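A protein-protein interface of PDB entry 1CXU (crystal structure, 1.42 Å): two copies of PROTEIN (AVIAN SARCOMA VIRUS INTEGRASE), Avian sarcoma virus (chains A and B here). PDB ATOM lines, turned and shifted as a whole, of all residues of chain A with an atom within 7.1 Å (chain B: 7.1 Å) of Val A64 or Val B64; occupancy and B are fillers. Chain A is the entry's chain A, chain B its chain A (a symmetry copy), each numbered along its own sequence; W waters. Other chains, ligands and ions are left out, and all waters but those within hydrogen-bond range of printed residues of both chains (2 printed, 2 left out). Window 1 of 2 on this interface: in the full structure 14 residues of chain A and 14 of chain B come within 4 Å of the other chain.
Ile A62 touches Tyr B147, and with the chains exchanged Tyr A147 touches Ile B62. Ala A63 touches Ala B143, and with the chains exchanged Ala A143 touches Ala B63. Ala A63 touches Met B146, and with the chains exchanged Met A146 touches Ala B63. Val A64 touches its own counterpart, Val B64. 17 positions are printed for both chains. Of the 9 pairs that touch across the chains among the printed residues, 9 have their exchanged pair printed and touching as well.
Among the printed residues, pairs that only touch across the chains: Ala A59 with Ala B143, Ile A62 with Tyr B147, Ala A63 with Ala B143, Ala A63 with Met B146, Val A64 with Val B64, Ala A143 with Ala B59, Ala A143 with Ala B63, Met A146 with Ala B63 and Tyr A147 with Ile B62.
Trp A58 touches none of the printed residues of chain B. Of the printed residues of chain B, Ala A59 touches Ala B143. Printed residues of chain B within 4 Å of Ile A62: Tyr B147. Printed residues of chain B within 4 Å of Ala A143: Ala B59 and Ala B63. Asn A150 touches none of the printed residues of chain B. Of chain A, only Val A64 (3.9 Å) comes within 4 Å of Val B64. Of the printed residues of chain A, Met B146 touches Ala A63. The nearest residue of chain A that does not touch Val B64 is Ala A63 (4.8 Å). The nearest printed residue of chain B that does not touch Ala A63 is Tyr B147 (4.4 Å).
O of Met B146 sits at hydrogen-bond distance from ND2 of Asn B150. The backbone carbonyl oxygen (O) of Met A146 is in hydrogen-bond range of the side-chain amide nitrogen (ND2) of Asn A150 (3.4 Å).
Hydrophobic or aromatic side chains of chain A within 4 Å of the printed part of chain B: Ile A62, Ala A63, Val A64, Ala A143, Met A146 and Tyr A147. Of the 17 printed residues of chain B, 7 touch a printed residue of chain A. Hydrophobic or aromatic side chains of chain B that line the printed part of chain A: Ile B62, Ala B63, Val B64, Ala B143, Met B146 and Tyr B147. Among the printed residues, 9 pairs touch across the chains.
Water W2 lies within hydrogen-bond range of the backbone carbonyl oxygen of Ala A63 (2.6 Å), the backbone NH of Tyr B147 (3.2 Å), the backbone carbonyl oxygen of Met B146 (3.4 Å) and the side-chain amide nitrogen of Asn B150 (3.4 Å). Water W1 lies within hydrogen-bond range of the backbone carbonyl oxygen (O) of Ala B63, the backbone NH (N) of Tyr A147, the backbone carbonyl oxygen (O) of Met A146 and the side-chain amide nitrogen (ND2) of Asn A150.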
ATOM      1  N   TRP A  14       9.825 -11.260  36.678  1.00  0.00           N
ATOM      2  CA  TRP A  14       9.984  -9.837  36.919  1.00  0.00           C
ATOM      3  C   TRP A  14       8.956  -9.293  37.881  1.00  0.00           C
ATOM      4  O   TRP A  14       7.855  -9.885  38.035  1.00  0.00           O
ATOM      5  CB  TRP A  14       9.764  -9.077  35.581  1.00  0.00           C
ATOM      6  CG  TRP A  14      10.767  -9.319  34.497  1.00  0.00           C
ATOM      7  CD1 TRP A  14      11.950  -9.999  34.520  1.00  0.00           C
ATOM      8  CD2 TRP A  14      10.656  -8.834  33.131  1.00  0.00           C
ATOM      9  NE1 TRP A  14      12.604  -9.991  33.305  1.00  0.00           N
ATOM     10  CE2 TRP A  14      11.799  -9.273  32.444  1.00  0.00           C
ATOM     11  CE3 TRP A  14       9.649  -8.063  32.494  1.00  0.00           C
ATOM     12  CZ2 TRP A  14      11.986  -8.959  31.072  1.00  0.00           C
ATOM     13  CZ3 TRP A  14       9.867  -7.776  31.132  1.00  0.00           C
ATOM     14  CH2 TRP A  14      10.997  -8.217  30.466  1.00  0.00           C
ATOM     15  N   ALA A  40      18.589  -6.746  38.059  1.00  0.00           N
ATOM     16  CA  ALA A  40      18.697  -5.742  36.997  1.00  0.00           C
ATOM     17  C   ALA A  40      17.377  -4.958  36.837  1.00  0.00           C
ATOM     18  O   ALA A  40      16.290  -5.516  36.981  1.00  0.00           O
ATOM     19  CB  ALA A  40      19.041  -6.380  35.655  1.00  0.00           C
ATOM     20  N   ILE A  41      17.521  -3.677  36.562  1.00  0.00           N
ATOM     21  CA  ILE A  41      16.398  -2.758  36.381  1.00  0.00           C
ATOM     22  C   ILE A  41      16.320  -2.233  34.949  1.00  0.00           C
ATOM     23  O   ILE A  41      17.326  -1.897  34.293  1.00  0.00           O
ATOM     24  CB  ILE A  41      16.576  -1.572  37.336  1.00  0.00           C
ATOM     25  CG1 ILE A  41      16.481  -2.060  38.802  1.00  0.00           C
ATOM     26  CG2 ILE A  41      15.676  -0.380  37.082  1.00  0.00           C
ATOM     27  CD1 ILE A  41      17.330  -1.099  39.666  1.00  0.00           C
ATOM     28  N   VAL A  42      15.070  -2.173  34.458  1.00  0.00           N
ATOM     29  CA  VAL A  42      14.784  -1.439  33.231  1.00  0.00           C
ATOM     30  C   VAL A  42      13.807  -0.319  33.560  1.00  0.00           C
ATOM     31  O   VAL A  42      12.814  -0.588  34.253  1.00  0.00           O
ATOM     32  CB  VAL A  42      14.140  -2.299  32.124  1.00  0.00           C
ATOM     33  CG1 VAL A  42      13.776  -1.439  30.894  1.00  0.00           C
ATOM     34  CG2 VAL A  42      15.051  -3.435  31.716  1.00  0.00           C
ATOM     35  N   TRP A  58       7.163  -3.020  28.705  1.00  0.00           N
ATOM     36  CA  TRP A  58       7.627  -4.395  28.637  1.00  0.00           C
ATOM     37  C   TRP A  58       8.268  -4.728  27.274  1.00  0.00           C
ATOM     38  O   TRP A  58       9.237  -5.519  27.274  1.00  0.00           O
ATOM     39  CB  TRP A  58       6.462  -5.332  28.973  1.00  0.00           C
ATOM     40  CG  TRP A  58       6.035  -5.383  30.422  1.00  0.00           C
ATOM     41  CD1 TRP A  58       6.848  -5.316  31.537  1.00  0.00           C
ATOM     42  CD2 TRP A  58       4.690  -5.540  30.920  1.00  0.00           C
ATOM     43  NE1 TRP A  58       6.062  -5.414  32.680  1.00  0.00           N
ATOM     44  CE2 TRP A  58       4.745  -5.551  32.318  1.00  0.00           C
ATOM     45  CE3 TRP A  58       3.463  -5.668  30.284  1.00  0.00           C
ATOM     46  CZ2 TRP A  58       3.603  -5.688  33.121  1.00  0.00           C
ATOM     47  CZ3 TRP A  58       2.324  -5.796  31.091  1.00  0.00           C
ATOM     48  CH2 TRP A  58       2.405  -5.801  32.498  1.00  0.00           C
ATOM     49  N   ALA A  59       7.795  -4.113  26.180  1.00  0.00           N
ATOM     50  CA  ALA A  59       8.488  -4.377  24.908  1.00  0.00           C
ATOM     51  C   ALA A  59       9.966  -3.966  24.937  1.00  0.00           C
ATOM     52  O   ALA A  59      10.879  -4.668  24.510  1.00  0.00           O
ATOM     53  CB  ALA A  59       7.759  -3.648  23.806  1.00  0.00           C
ATOM     54  N   THR A  60      10.180  -2.764  25.528  1.00  0.00           N
ATOM     55  CA  THR A  60      11.567  -2.326  25.736  1.00  0.00           C
ATOM     56  C   THR A  60      12.362  -3.272  26.661  1.00  0.00           C
ATOM     57  O   THR A  60      13.513  -3.620  26.364  1.00  0.00           O
ATOM     58  CB  THR A  60      11.585  -0.904  26.330  1.00  0.00           C
ATOM     59  OG1 THR A  60      10.967  -0.036  25.348  1.00  0.00           O
ATOM     60  CG2 THR A  60      13.006  -0.394  26.535  1.00  0.00           C
ATOM     61  N   ALA A  61      11.719  -3.626  27.779  1.00  0.00           N
ATOM     62  CA  ALA A  61      12.374  -4.505  28.755  1.00  0.00           C
ATOM     63  C   ALA A  61      12.717  -5.856  28.132  1.00  0.00           C
ATOM     64  O   ALA A  61      13.777  -6.388  28.421  1.00  0.00           O
ATOM     65  CB  ALA A  61      11.513  -4.656  30.017  1.00  0.00           C
ATOM     66  N   ILE A  62      11.865  -6.389  27.220  1.00  0.00           N
ATOM     67  CA  ILE A  62      12.219  -7.672  26.565  1.00  0.00           C
ATOM     68  C   ILE A  62      13.463  -7.502  25.682  1.00  0.00           C
ATOM     69  O   ILE A  62      14.317  -8.364  25.622  1.00  0.00           O
ATOM     70  CB  ILE A  62      10.974  -8.156  25.808  1.00  0.00           C
ATOM     71  CG1 ILE A  62       9.873  -8.580  26.800  1.00  0.00           C
ATOM     72  CG2 ILE A  62      11.280  -9.278  24.843  1.00  0.00           C
ATOM     73  CD1 ILE A  62       8.548  -8.818  26.097  1.00  0.00           C
ATOM     74  N   ALA A  63      13.590  -6.341  25.009  1.00  0.00           N
ATOM     75  CA  ALA A  63      14.753  -6.085  24.147  1.00  0.00           C
ATOM     76  C   ALA A  63      16.041  -5.924  24.943  1.00  0.00           C
ATOM     77  O   ALA A  63      17.128  -6.177  24.410  1.00  0.00           O
ATOM     78  CB  ALA A  63      14.551  -4.819  23.308  1.00  0.00           C
ATOM     79  N   VAL A  64      15.930  -5.500  26.215  1.00  0.00           N
ATOM     80  CA  VAL A  64      17.100  -5.349  27.066  1.00  0.00           C
ATOM     81  C   VAL A  64      17.502  -6.622  27.809  1.00  0.00           C
ATOM     82  O   VAL A  64      18.710  -6.932  27.869  1.00  0.00           O
ATOM     83  CB  VAL A  64      16.887  -4.220  28.090  1.00  0.00           C
ATOM     84  CG1 VAL A  64      18.065  -4.102  29.042  1.00  0.00           C
ATOM     85  CG2 VAL A  64      16.622  -2.893  27.349  1.00  0.00           C
ATOM     86  N   LEU A  65      16.497  -7.307  28.382  1.00  0.00           N
ATOM     87  CA  LEU A  65      16.756  -8.412  29.298  1.00  0.00           C
ATOM     88  C   LEU A  65      16.426  -9.788  28.690  1.00  0.00           C
ATOM     89  O   LEU A  65      16.911 -10.777  29.280  1.00  0.00           O
ATOM     90  CB  LEU A  65      15.898  -8.305  30.565  1.00  0.00           C
ATOM     91  CG  LEU A  65      16.005  -7.016  31.377  1.00  0.00           C
ATOM     92  CD1 LEU A  65      14.943  -6.998  32.474  1.00  0.00           C
ATOM     93  CD2 LEU A  65      17.399  -6.879  31.975  1.00  0.00           C
ATOM     94  N   GLY A  66      15.636  -9.852  27.652  1.00  0.00           N
ATOM     95  CA  GLY A  66      15.101 -11.122  27.162  1.00  0.00           C
ATOM     96  C   GLY A  66      13.668 -11.302  27.601  1.00  0.00           C
ATOM     97  O   GLY A  66      13.059 -10.514  28.364  1.00  0.00           O
ATOM     98  N   ALA A 143      18.927   7.197  31.149  1.00  0.00           N
ATOM     99  CA  ALA A 143      19.763   6.072  30.696  1.00  0.00           C
ATOM    100  C   ALA A 143      21.043   5.995  31.524  1.00  0.00           C
ATOM    101  O   ALA A 143      21.496   4.877  31.819  1.00  0.00           O
ATOM    102  CB  ALA A 143      20.076   6.209  29.215  1.00  0.00           C
ATOM    103  N   MET A 146      19.987   4.356  34.855  1.00  0.00           N
ATOM    104  CA  MET A 146      19.817   2.892  34.677  1.00  0.00           C
ATOM    105  C   MET A 146      21.185   2.234  34.570  1.00  0.00           C
ATOM    106  O   MET A 146      21.361   1.218  35.305  1.00  0.00           O
ATOM    107  CB  MET A 146      18.956   2.682  33.432  1.00  0.00           C
ATOM    108  CG  MET A 146      18.717   1.184  33.126  1.00  0.00           C
ATOM    109  SD  MET A 146      17.598   1.053  31.721  1.00  0.00           S
ATOM    110  CE  MET A 146      18.042  -0.610  31.178  1.00  0.00           C
ATOM    111  N   TYR A 147      22.087   2.773  33.779  1.00  0.00           N
ATOM    112  CA  TYR A 147      23.472   2.242  33.720  1.00  0.00           C
ATOM    113  C   TYR A 147      24.100   2.180  35.100  1.00  0.00           C
ATOM    114  O   TYR A 147      24.634   1.148  35.562  1.00  0.00           O
ATOM    115  CB  TYR A 147      24.331   3.045  32.768  1.00  0.00           C
ATOM    116  CG  TYR A 147      25.832   2.875  32.931  1.00  0.00           C
ATOM    117  CD1 TYR A 147      26.502   1.746  32.446  1.00  0.00           C
ATOM    118  CD2 TYR A 147      26.620   3.818  33.586  1.00  0.00           C
ATOM    119  CE1 TYR A 147      27.883   1.590  32.609  1.00  0.00           C
ATOM    120  CE2 TYR A 147      27.993   3.690  33.751  1.00  0.00           C
ATOM    121  CZ  TYR A 147      28.600   2.566  33.253  1.00  0.00           C
ATOM    122  OH  TYR A 147      29.991   2.447  33.425  1.00  0.00           O
ATOM    123  N   ASN A 150      22.702  -0.601  37.442  1.00  0.00           N
ATOM    124  CA  ASN A 150      22.944  -1.969  36.956  1.00  0.00           C
ATOM    125  C   ASN A 150      24.409  -2.378  36.997  1.00  0.00           C
ATOM    126  O   ASN A 150      24.800  -3.515  36.682  1.00  0.00           O
ATOM    127  CB  ASN A 150      22.423  -2.103  35.524  1.00  0.00           C
ATOM    128  CG  ASN A 150      20.886  -2.177  35.545  1.00  0.00           C
ATOM    129  OD1 ASN A 150      20.309  -2.505  36.564  1.00  0.00           O
ATOM    130  ND2 ASN A 150      20.325  -1.880  34.389  1.00  0.00           N
ATOM    131  N   TRP B  14      32.798  -1.458  19.928  1.00  0.00           N
ATOM    132  CA  TRP B  14      31.596  -1.414  19.115  1.00  0.00           C
ATOM    133  C   TRP B  14      31.852  -0.873  17.730  1.00  0.00           C
ATOM    134  O   TRP B  14      32.841  -0.123  17.514  1.00  0.00           O
ATOM    135  CB  TRP B  14      30.581  -0.439  19.776  1.00  0.00           C
ATOM    136  CG  TRP B  14      30.035  -0.839  21.111  1.00  0.00           C
ATOM    137  CD1 TRP B  14      30.166  -2.005  21.808  1.00  0.00           C
ATOM    138  CD2 TRP B  14      29.205  -0.001  21.960  1.00  0.00           C
ATOM    139  NE1 TRP B  14      29.497  -1.993  23.015  1.00  0.00           N
ATOM    140  CE2 TRP B  14      28.907  -0.749  23.111  1.00  0.00           C
ATOM    141  CE3 TRP B  14      28.723   1.322  21.780  1.00  0.00           C
ATOM    142  CZ2 TRP B  14      28.105  -0.198  24.145  1.00  0.00           C
ATOM    143  CZ3 TRP B  14      27.936   1.835  22.830  1.00  0.00           C
ATOM    144  CH2 TRP B  14      27.651   1.088  23.960  1.00  0.00           C
ATOM    145  N   ALA B  40      25.970  -8.696  19.610  1.00  0.00           N
ATOM    146  CA  ALA B  40      24.712  -8.080  20.041  1.00  0.00           C
ATOM    147  C   ALA B  40      24.500  -6.711  19.360  1.00  0.00           C
ATOM    148  O   ALA B  40      25.451  -5.962  19.142  1.00  0.00           O
ATOM    149  CB  ALA B  40      24.676  -7.876  21.552  1.00  0.00           C
ATOM    150  N   ILE B  41      23.254  -6.442  19.030  1.00  0.00           N
ATOM    151  CA  ILE B  41      22.842  -5.204  18.370  1.00  0.00           C
ATOM    152  C   ILE B  41      21.943  -4.354  19.265  1.00  0.00           C
ATOM    153  O   ILE B  41      21.043  -4.839  19.980  1.00  0.00           O
ATOM    154  CB  ILE B  41      22.075  -5.561  17.091  1.00  0.00           C
ATOM    155  CG1 ILE B  41      23.022  -6.270  16.092  1.00  0.00           C
ATOM    156  CG2 ILE B  41      21.319  -4.423  16.437  1.00  0.00           C
ATOM    157  CD1 ILE B  41      22.155  -7.207  15.219  1.00  0.00           C
ATOM    158  N   VAL B  42      22.214  -3.038  19.219  1.00  0.00           N
ATOM    159  CA  VAL B  42      21.285  -2.064  19.780  1.00  0.00           C
ATOM    160  C   VAL B  42      20.816  -1.150  18.657  1.00  0.00           C
ATOM    161  O   VAL B  42      21.666  -0.680  17.885  1.00  0.00           O
ATOM    162  CB  VAL B  42      21.904  -1.168  20.873  1.00  0.00           C
ATOM    163  CG1 VAL B  42      20.896  -0.099  21.350  1.00  0.00           C
ATOM    164  CG2 VAL B  42      22.387  -1.992  22.045  1.00  0.00           C
ATOM    165  N   TRP B  58      24.098   6.278  21.667  1.00  0.00           N
ATOM    166  CA  TRP B  58      25.074   5.628  22.526  1.00  0.00           C
ATOM    167  C   TRP B  58      24.654   5.651  24.009  1.00  0.00           C
ATOM    168  O   TRP B  58      24.955   4.657  24.706  1.00  0.00           O
ATOM    169  CB  TRP B  58      26.444   6.277  22.303  1.00  0.00           C
ATOM    170  CG  TRP B  58      27.140   5.950  21.000  1.00  0.00           C
ATOM    171  CD1 TRP B  58      27.139   4.742  20.331  1.00  0.00           C
ATOM    172  CD2 TRP B  58      27.966   6.837  20.218  1.00  0.00           C
ATOM    173  NE1 TRP B  58      27.912   4.858  19.181  1.00  0.00           N
ATOM    174  CE2 TRP B  58      28.422   6.130  19.100  1.00  0.00           C
ATOM    175  CE3 TRP B  58      28.341   8.162  20.387  1.00  0.00           C
ATOM    176  CZ2 TRP B  58      29.253   6.703  18.127  1.00  0.00           C
ATOM    177  CZ3 TRP B  58      29.165   8.734  19.407  1.00  0.00           C
ATOM    178  CH2 TRP B  58      29.608   8.001  18.288  1.00  0.00           C
ATOM    179  N   ALA B  59      23.945   6.699  24.455  1.00  0.00           N
ATOM    180  CA  ALA B  59      23.475   6.649  25.849  1.00  0.00           C
ATOM    181  C   ALA B  59      22.555   5.451  26.127  1.00  0.00           C
ATOM    182  O   ALA B  59      22.659   4.725  27.112  1.00  0.00           O
ATOM    183  CB  ALA B  59      22.764   7.943  26.162  1.00  0.00           C
ATOM    184  N   THR B  60      21.639   5.238  25.150  1.00  0.00           N
ATOM    185  CA  THR B  60      20.792   4.041  25.239  1.00  0.00           C
ATOM    186  C   THR B  60      21.603   2.728  25.195  1.00  0.00           C
ATOM    187  O   THR B  60      21.353   1.809  25.987  1.00  0.00           O
ATOM    188  CB  THR B  60      19.764   4.038  24.091  1.00  0.00           C
ATOM    189  OG1 THR B  60      18.931   5.210  24.277  1.00  0.00           O
ATOM    190  CG2 THR B  60      18.841   2.829  24.159  1.00  0.00           C
ATOM    191  N   ALA B  61      22.531   2.680  24.234  1.00  0.00           N
ATOM    192  CA  ALA B  61      23.357   1.477  24.070  1.00  0.00           C
ATOM    193  C   ALA B  61      24.174   1.198  25.330  1.00  0.00           C
ATOM    194  O   ALA B  61      24.313   0.043  25.699  1.00  0.00           O
ATOM    195  CB  ALA B  61      24.245   1.591  22.822  1.00  0.00           C
ATOM    196  N   ILE B  62      24.658   2.249  26.039  1.00  0.00           N
ATOM    197  CA  ILE B  62      25.401   1.989  27.297  1.00  0.00           C
ATOM    198  C   ILE B  62      24.475   1.372  28.354  1.00  0.00           C
ATOM    199  O   ILE B  62      24.861   0.490  29.095  1.00  0.00           O
ATOM    200  CB  ILE B  62      26.049   3.312  27.726  1.00  0.00           C
ATOM    201  CG1 ILE B  62      27.173   3.703  26.747  1.00  0.00           C
ATOM    202  CG2 ILE B  62      26.569   3.273  29.144  1.00  0.00           C
ATOM    203  CD1 ILE B  62      27.659   5.121  26.990  1.00  0.00           C
ATOM    204  N   ALA B  63      23.203   1.819  28.399  1.00  0.00           N
ATOM    205  CA  ALA B  63      22.242   1.280  29.372  1.00  0.00           C
ATOM    206  C   ALA B  63      21.869  -0.166  29.078  1.00  0.00           C
ATOM    207  O   ALA B  63      21.483  -0.900  29.996  1.00  0.00           O
ATOM    208  CB  ALA B  63      20.955   2.109  29.393  1.00  0.00           C
ATOM    209  N   VAL B  64      21.974  -0.582  27.802  1.00  0.00           N
ATOM    210  CA  VAL B  64      21.673  -1.955  27.428  1.00  0.00           C
ATOM    211  C   VAL B  64      22.857  -2.913  27.556  1.00  0.00           C
ATOM    212  O   VAL B  64      22.672  -4.041  28.057  1.00  0.00           O
ATOM    213  CB  VAL B  64      21.130  -2.022  25.990  1.00  0.00           C
ATOM    214  CG1 VAL B  64      20.889  -3.456  25.551  1.00  0.00           C
ATOM    215  CG2 VAL B  64      19.847  -1.172  25.882  1.00  0.00           C
ATOM    216  N   LEU B  65      24.028  -2.461  27.074  1.00  0.00           N
ATOM    217  CA  LEU B  65      25.182  -3.343  26.932  1.00  0.00           C
ATOM    218  C   LEU B  65      26.287  -3.057  27.966  1.00  0.00           C
ATOM    219  O   LEU B  65      27.144  -3.955  28.112  1.00  0.00           O
ATOM    220  CB  LEU B  65      25.849  -3.181  25.561  1.00  0.00           C
ATOM    221  CG  LEU B  65      24.973  -3.389  24.327  1.00  0.00           C
ATOM    222  CD1 LEU B  65      25.739  -2.991  23.067  1.00  0.00           C
ATOM    223  CD2 LEU B  65      24.512  -4.838  24.241  1.00  0.00           C
ATOM    224  N   GLY B  66      26.303  -1.904  28.579  1.00  0.00           N
ATOM    225  CA  GLY B  66      27.437  -1.476  29.397  1.00  0.00           C
ATOM    226  C   GLY B  66      28.297  -0.491  28.644  1.00  0.00           C
ATOM    227  O   GLY B  66      28.114  -0.165  27.447  1.00  0.00           O
ATOM    228  N   ALA B 143      11.565  -2.857  18.802  1.00  0.00           N
ATOM    229  CA  ALA B 143      12.052  -3.593  19.981  1.00  0.00           C
ATOM    230  C   ALA B 143      11.897  -5.097  19.769  1.00  0.00           C
ATOM    231  O   ALA B 143      12.777  -5.854  20.207  1.00  0.00           O
ATOM    232  CB  ALA B 143      11.317  -3.136  21.230  1.00  0.00           C
ATOM    233  N   MET B 146      14.829  -6.097  17.469  1.00  0.00           N
ATOM    234  CA  MET B 146      16.092  -6.169  18.245  1.00  0.00           C
ATOM    235  C   MET B 146      16.087  -7.428  19.101  1.00  0.00           C
ATOM    236  O   MET B 146      17.136  -8.134  19.038  1.00  0.00           O
ATOM    237  CB  MET B 146      16.191  -4.888  19.073  1.00  0.00           C
ATOM    238  CG  MET B 146      17.467  -4.847  19.948  1.00  0.00           C
ATOM    239  SD  MET B 146      17.545  -3.253  20.782  1.00  0.00           S
ATOM    240  CE  MET B 146      18.617  -3.722  22.156  1.00  0.00           C
ATOM    241  N   TYR B 147      15.008  -7.718  19.794  1.00  0.00           N
ATOM    242  CA  TYR B 147      14.904  -8.988  20.556  1.00  0.00           C
ATOM    243  C   TYR B 147      15.174 -10.190  19.669  1.00  0.00           C
ATOM    244  O   TYR B 147      16.006 -11.077  19.957  1.00  0.00           O
ATOM    245  CB  TYR B 147      13.562  -9.111  21.243  1.00  0.00           C
ATOM    246  CG  TYR B 147      13.177 -10.511  21.692  1.00  0.00           C
ATOM    247  CD1 TYR B 147      13.721 -11.090  22.844  1.00  0.00           C
ATOM    248  CD2 TYR B 147      12.280 -11.301  20.977  1.00  0.00           C
ATOM    249  CE1 TYR B 147      13.371 -12.384  23.247  1.00  0.00           C
ATOM    250  CE2 TYR B 147      11.909 -12.583  21.363  1.00  0.00           C
ATOM    251  CZ  TYR B 147      12.470 -13.100  22.502  1.00  0.00           C
ATOM    252  OH  TYR B 147      12.088 -14.399  22.883  1.00  0.00           O
ATOM    253  N   ASN B 150      18.889 -10.666  18.599  1.00  0.00           N
ATOM    254  CA  ASN B 150      19.805 -10.927  19.720  1.00  0.00           C
ATOM    255  C   ASN B 150      19.599 -12.287  20.370  1.00  0.00           C
ATOM    256  O   ASN B 150      20.316 -12.709  21.293  1.00  0.00           O
ATOM    257  CB  ASN B 150      19.644  -9.834  20.778  1.00  0.00           C
ATOM    258  CG  ASN B 150      20.314  -8.540  20.281  1.00  0.00           C
ATOM    259  OD1 ASN B 150      21.161  -8.593  19.410  1.00  0.00           O
ATOM    260  ND2 ASN B 150      19.891  -7.454  20.897  1.00  0.00           N
HETATM  261  O   HOH W   1      22.377  -0.079  32.317  1.00  0.00           O
HETATM  262  O   HOH W   2      16.852  -7.867  22.427  1.00  0.00           O
